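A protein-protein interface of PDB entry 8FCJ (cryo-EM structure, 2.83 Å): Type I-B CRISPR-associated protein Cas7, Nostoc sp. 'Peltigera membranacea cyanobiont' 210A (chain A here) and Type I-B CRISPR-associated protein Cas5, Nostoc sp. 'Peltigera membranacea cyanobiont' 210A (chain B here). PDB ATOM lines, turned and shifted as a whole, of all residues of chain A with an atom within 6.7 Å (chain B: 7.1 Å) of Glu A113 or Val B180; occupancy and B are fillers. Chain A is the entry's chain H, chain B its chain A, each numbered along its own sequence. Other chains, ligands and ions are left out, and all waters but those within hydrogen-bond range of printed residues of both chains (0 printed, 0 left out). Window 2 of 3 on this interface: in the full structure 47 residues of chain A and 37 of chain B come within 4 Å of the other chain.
OE2 of Glu A115 sits close to OD1 of Asp B178, 3.3 Å away. ND1 of His B179 sits at hydrogen-bond distance from OE1 of Glu A115.
The side-chain carboxylate (OD1) of Asp B178 is in hydrogen-bond range of the backbone NH (N) of Val B180 (2.7 Å). The backbone NH (N) of Asp B178 sits at hydrogen-bond distance from the side-chain hydroxyl (OG1) of Thr B185, 2.9 Å away. The side-chain carboxylate (OD1) of Asp B178 sits at hydrogen-bond distance from the backbone NH (N) of Gly B181 (3.2 Å). OD2 of Asp B178 is in hydrogen-bond range of N of Arg B183, 3.4 Å away.
Ala A112 touches Val B180 (O to CA, 3.9 Å). CG1 of Val B180 touches CA of Glu A113, 3.9 Å away. Thr A114 touches Val B180 (C to CG2, 3.6 Å). Glu A115 touches Val B177 (OE2 to O, 3.9 Å).
Leu A109 touches none of the printed residues of chain B. Printed residues of chain B within 4 Å of Thr A114: Val B180 (3.6 Å). Printed residues of chain B within 4 Å of Glu A115: Val B177, Asp B178 and His B179. Asn A134 touches none of the printed residues of chain B. Of the printed residues of chain A, Asp B178 touches Glu A115 (3.3 Å). Of the printed residues of chain A, Val B180 touches Ala A112 (3.9 Å), Glu A113 (3.9 Å) and Thr A114 (3.6 Å). The nearest printed residue of chain A that does not touch Val B180 is Glu A115 (4.01 Å). The nearest printed residue of chain A that does not touch Val B177 is Thr A114 (9.0 Å).
Of the 9 printed residues of chain A, 4 touch a printed residue of chain B. Printed residues of chain A that touch a printed residue of chain B: Ala A112, Glu A113, Thr A114 and Glu A115. Of the 9 printed residues of chain B, 4 touch a printed residue of chain A. Printed residues of chain B that touch a printed residue of chain A: Val B177, Asp B178, His B179 and Val B180.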
ATOM      1  N   LEU A 108     -21.818  -3.196  -5.796  1.00  0.00           N
ATOM      2  CA  LEU A 108     -21.831  -3.132  -4.343  1.00  0.00           C
ATOM      3  C   LEU A 108     -21.133  -1.868  -3.853  1.00  0.00           C
ATOM      4  O   LEU A 108     -20.545  -1.109  -4.625  1.00  0.00           O
ATOM      5  CB  LEU A 108     -21.169  -4.375  -3.745  1.00  0.00           C
ATOM      6  CG  LEU A 108     -22.064  -5.607  -3.624  1.00  0.00           C
ATOM      7  CD1 LEU A 108     -21.238  -6.833  -3.287  1.00  0.00           C
ATOM      8  CD2 LEU A 108     -23.137  -5.378  -2.578  1.00  0.00           C
ATOM      9  N   LEU A 109     -21.213  -1.649  -2.540  1.00  0.00           N
ATOM     10  CA  LEU A 109     -20.594  -0.469  -1.946  1.00  0.00           C
ATOM     11  C   LEU A 109     -19.083  -0.482  -2.136  1.00  0.00           C
ATOM     12  O   LEU A 109     -18.484   0.545  -2.474  1.00  0.00           O
ATOM     13  CB  LEU A 109     -20.939  -0.388  -0.461  1.00  0.00           C
ATOM     14  CG  LEU A 109     -20.141   0.642   0.336  1.00  0.00           C
ATOM     15  CD1 LEU A 109     -20.511   2.039  -0.108  1.00  0.00           C
ATOM     16  CD2 LEU A 109     -20.370   0.474   1.826  1.00  0.00           C
ATOM     17  N   GLU A 110     -18.449  -1.636  -1.926  1.00  0.00           N
ATOM     18  CA  GLU A 110     -17.002  -1.725  -2.064  1.00  0.00           C
ATOM     19  C   GLU A 110     -16.552  -1.586  -3.510  1.00  0.00           C
ATOM     20  O   GLU A 110     -15.363  -1.366  -3.756  1.00  0.00           O
ATOM     21  CB  GLU A 110     -16.496  -3.048  -1.488  1.00  0.00           C
ATOM     22  CG  GLU A 110     -16.773  -3.228  -0.007  1.00  0.00           C
ATOM     23  CD  GLU A 110     -18.172  -3.744   0.267  1.00  0.00           C
ATOM     24  OE1 GLU A 110     -18.803  -4.278  -0.668  1.00  0.00           O
ATOM     25  OE2 GLU A 110     -18.642  -3.613   1.417  1.00  0.00           O
ATOM     26  N   SER A 111     -17.471  -1.714  -4.467  1.00  0.00           N
ATOM     27  CA  SER A 111     -17.115  -1.570  -5.873  1.00  0.00           C
ATOM     28  C   SER A 111     -16.695  -0.152  -6.225  1.00  0.00           C
ATOM     29  O   SER A 111     -15.993   0.042  -7.223  1.00  0.00           O
ATOM     30  CB  SER A 111     -18.287  -1.991  -6.755  1.00  0.00           C
ATOM     31  OG  SER A 111     -18.376  -1.156  -7.892  1.00  0.00           O
ATOM     32  N   ALA A 112     -17.109   0.841  -5.440  1.00  0.00           N
ATOM     33  CA  ALA A 112     -16.792   2.228  -5.739  1.00  0.00           C
ATOM     34  C   ALA A 112     -15.540   2.726  -5.031  1.00  0.00           C
ATOM     35  O   ALA A 112     -15.011   3.776  -5.410  1.00  0.00           O
ATOM     36  CB  ALA A 112     -17.971   3.132  -5.368  1.00  0.00           C
ATOM     37  N   GLU A 113     -15.054   2.004  -4.022  1.00  0.00           N
ATOM     38  CA  GLU A 113     -13.876   2.412  -3.266  1.00  0.00           C
ATOM     39  C   GLU A 113     -12.682   1.502  -3.532  1.00  0.00           C
ATOM     40  O   GLU A 113     -11.804   1.354  -2.679  1.00  0.00           O
ATOM     41  CB  GLU A 113     -14.187   2.457  -1.771  1.00  0.00           C
ATOM     42  CG  GLU A 113     -15.186   1.418  -1.307  1.00  0.00           C
ATOM     43  CD  GLU A 113     -15.535   1.567   0.159  1.00  0.00           C
ATOM     44  OE1 GLU A 113     -15.472   2.702   0.674  1.00  0.00           O
ATOM     45  OE2 GLU A 113     -15.871   0.549   0.799  1.00  0.00           O
ATOM     46  N   THR A 114     -12.636   0.884  -4.709  1.00  0.00           N
ATOM     47  CA  THR A 114     -11.505   0.055  -5.095  1.00  0.00           C
ATOM     48  C   THR A 114     -11.405   0.040  -6.612  1.00  0.00           C
ATOM     49  O   THR A 114     -12.358   0.372  -7.321  1.00  0.00           O
ATOM     50  CB  THR A 114     -11.630  -1.373  -4.552  1.00  0.00           C
ATOM     51  OG1 THR A 114     -10.357  -2.024  -4.625  1.00  0.00           O
ATOM     52  CG2 THR A 114     -12.638  -2.162  -5.361  1.00  0.00           C
ATOM     53  N   GLU A 115     -10.230  -0.343  -7.107  1.00  0.00           N
ATOM     54  CA  GLU A 115      -9.998  -0.378  -8.544  1.00  0.00           C
ATOM     55  C   GLU A 115     -10.248  -1.750  -9.150  1.00  0.00           C
ATOM     56  O   GLU A 115     -10.726  -1.838 -10.287  1.00  0.00           O
ATOM     57  CB  GLU A 115      -8.567   0.066  -8.857  1.00  0.00           C
ATOM     58  CG  GLU A 115      -8.346   1.566  -8.757  1.00  0.00           C
ATOM     59  CD  GLU A 115      -8.732   2.304 -10.026  1.00  0.00           C
ATOM     60  OE1 GLU A 115      -9.362   1.690 -10.912  1.00  0.00           O
ATOM     61  OE2 GLU A 115      -8.406   3.504 -10.136  1.00  0.00           O
ATOM     62  N   ASN A 134     -16.937  -8.263  -6.345  1.00  0.00           N
ATOM     63  CA  ASN A 134     -17.378  -6.943  -5.920  1.00  0.00           C
ATOM     64  C   ASN A 134     -18.493  -6.383  -6.789  1.00  0.00           C
ATOM     65  O   ASN A 134     -19.212  -5.483  -6.346  1.00  0.00           O
ATOM     66  CB  ASN A 134     -16.195  -5.975  -5.933  1.00  0.00           C
ATOM     67  CG  ASN A 134     -16.170  -5.078  -4.723  1.00  0.00           C
ATOM     68  OD1 ASN A 134     -16.963  -5.242  -3.798  1.00  0.00           O
ATOM     69  ND2 ASN A 134     -15.247  -4.126  -4.715  1.00  0.00           N
ATOM     70  N   ARG B  22     -19.196  15.457 -10.933  1.00  0.00           N
ATOM     71  CA  ARG B  22     -19.904  14.487 -10.112  1.00  0.00           C
ATOM     72  C   ARG B  22     -21.304  14.926  -9.722  1.00  0.00           C
ATOM     73  O   ARG B  22     -22.182  14.075  -9.577  1.00  0.00           O
ATOM     74  CB  ARG B  22     -19.103  14.180  -8.842  1.00  0.00           C
ATOM     75  CG  ARG B  22     -17.980  13.185  -9.066  1.00  0.00           C
ATOM     76  CD  ARG B  22     -16.715  13.605  -8.351  1.00  0.00           C
ATOM     77  NE  ARG B  22     -16.586  12.958  -7.052  1.00  0.00           N
ATOM     78  CZ  ARG B  22     -15.738  11.976  -6.788  1.00  0.00           C
ATOM     79  NH1 ARG B  22     -14.928  11.495  -7.716  1.00  0.00           N
ATOM     80  NH2 ARG B  22     -15.700  11.462  -5.562  1.00  0.00           N
ATOM     81  N   VAL B 177      -7.266   7.009 -15.671  1.00  0.00           N
ATOM     82  CA  VAL B 177      -8.395   7.363 -14.821  1.00  0.00           C
ATOM     83  C   VAL B 177      -8.295   6.591 -13.514  1.00  0.00           C
ATOM     84  O   VAL B 177      -8.099   5.371 -13.518  1.00  0.00           O
ATOM     85  CB  VAL B 177      -9.736   7.079 -15.520  1.00  0.00           C
ATOM     86  CG1 VAL B 177     -10.870   7.076 -14.516  1.00  0.00           C
ATOM     87  CG2 VAL B 177      -9.990   8.105 -16.602  1.00  0.00           C
ATOM     88  N   ASP B 178      -8.423   7.305 -12.399  1.00  0.00           N
ATOM     89  CA  ASP B 178      -8.550   6.702 -11.079  1.00  0.00           C
ATOM     90  C   ASP B 178     -10.037   6.723 -10.750  1.00  0.00           C
ATOM     91  O   ASP B 178     -10.617   7.792 -10.535  1.00  0.00           O
ATOM     92  CB  ASP B 178      -7.721   7.473 -10.049  1.00  0.00           C
ATOM     93  CG  ASP B 178      -8.020   7.077  -8.600  1.00  0.00           C
ATOM     94  OD1 ASP B 178      -8.920   6.256  -8.332  1.00  0.00           O
ATOM     95  OD2 ASP B 178      -7.333   7.610  -7.705  1.00  0.00           O
ATOM     96  N   HIS B 179     -10.654   5.544 -10.710  1.00  0.00           N
ATOM     97  CA  HIS B 179     -12.093   5.454 -10.511  1.00  0.00           C
ATOM     98  C   HIS B 179     -12.510   5.620  -9.057  1.00  0.00           C
ATOM     99  O   HIS B 179     -13.703   5.799  -8.792  1.00  0.00           O
ATOM    100  CB  HIS B 179     -12.605   4.119 -11.047  1.00  0.00           C
ATOM    101  CG  HIS B 179     -12.247   3.872 -12.477  1.00  0.00           C
ATOM    102  ND1 HIS B 179     -11.156   3.118 -12.851  1.00  0.00           N
ATOM    103  CD2 HIS B 179     -12.827   4.290 -13.625  1.00  0.00           C
ATOM    104  CE1 HIS B 179     -11.085   3.077 -14.170  1.00  0.00           C
ATOM    105  NE2 HIS B 179     -12.088   3.780 -14.663  1.00  0.00           N
ATOM    106  N   VAL B 180     -11.571   5.567  -8.115  1.00  0.00           N
ATOM    107  CA  VAL B 180     -11.920   5.749  -6.710  1.00  0.00           C
ATOM    108  C   VAL B 180     -12.012   7.230  -6.369  1.00  0.00           C
ATOM    109  O   VAL B 180     -13.076   7.736  -5.997  1.00  0.00           O
ATOM    110  CB  VAL B 180     -10.903   5.029  -5.808  1.00  0.00           C
ATOM    111  CG1 VAL B 180     -11.343   5.098  -4.358  1.00  0.00           C
ATOM    112  CG2 VAL B 180     -10.736   3.588  -6.252  1.00  0.00           C
ATOM    113  N   GLY B 181     -10.901   7.946  -6.504  1.00  0.00           N
ATOM    114  CA  GLY B 181     -10.890   9.377  -6.281  1.00  0.00           C
ATOM    115  C   GLY B 181     -10.389  10.125  -7.498  1.00  0.00           C
ATOM    116  O   GLY B 181     -10.941   9.984  -8.591  1.00  0.00           O
ATOM    117  N   SER B 182      -9.346  10.934  -7.317  1.00  0.00           N
ATOM    118  CA  SER B 182      -8.707  11.597  -8.445  1.00  0.00           C
ATOM    119  C   SER B 182      -7.189  11.629  -8.312  1.00  0.00           C
ATOM    120  O   SER B 182      -6.532  12.335  -9.087  1.00  0.00           O
ATOM    121  CB  SER B 182      -9.244  13.022  -8.611  1.00  0.00           C
ATOM    122  OG  SER B 182      -8.844  13.843  -7.528  1.00  0.00           O
ATOM    123  N   ARG B 183      -6.618  10.898  -7.355  1.00  0.00           N
ATOM    124  CA  ARG B 183      -5.182  10.975  -7.109  1.00  0.00           C
ATOM    125  C   ARG B 183      -4.381  10.449  -8.294  1.00  0.00           C
ATOM    126  O   ARG B 183      -3.399  11.069  -8.715  1.00  0.00           O
ATOM    127  CB  ARG B 183      -4.835  10.197  -5.842  1.00  0.00           C
ATOM    128  CG  ARG B 183      -3.369  10.237  -5.466  1.00  0.00           C
ATOM    129  CD  ARG B 183      -3.188  10.114  -3.964  1.00  0.00           C
ATOM    130  NE  ARG B 183      -4.106   9.144  -3.380  1.00  0.00           N
ATOM    131  CZ  ARG B 183      -3.979   7.829  -3.489  1.00  0.00           C
ATOM    132  NH1 ARG B 183      -2.973   7.283  -4.152  1.00  0.00           N
ATOM    133  NH2 ARG B 183      -4.885   7.040  -2.916  1.00  0.00           N
ATOM    134  N   THR B 185      -5.473   9.928 -11.422  1.00  0.00           N
ATOM    135  CA  THR B 185      -5.904  10.382 -12.736  1.00  0.00           C
ATOM    136  C   THR B 185      -4.864  11.326 -13.326  1.00  0.00           C
ATOM    137  O   THR B 185      -4.391  12.244 -12.651  1.00  0.00           O
ATOM    138  CB  THR B 185      -7.258  11.078 -12.640  1.00  0.00           C
ATOM    139  OG1 THR B 185      -8.206  10.194 -12.033  1.00  0.00           O
ATOM    140  CG2 THR B 185      -7.755  11.463 -14.018  1.00  0.00           C
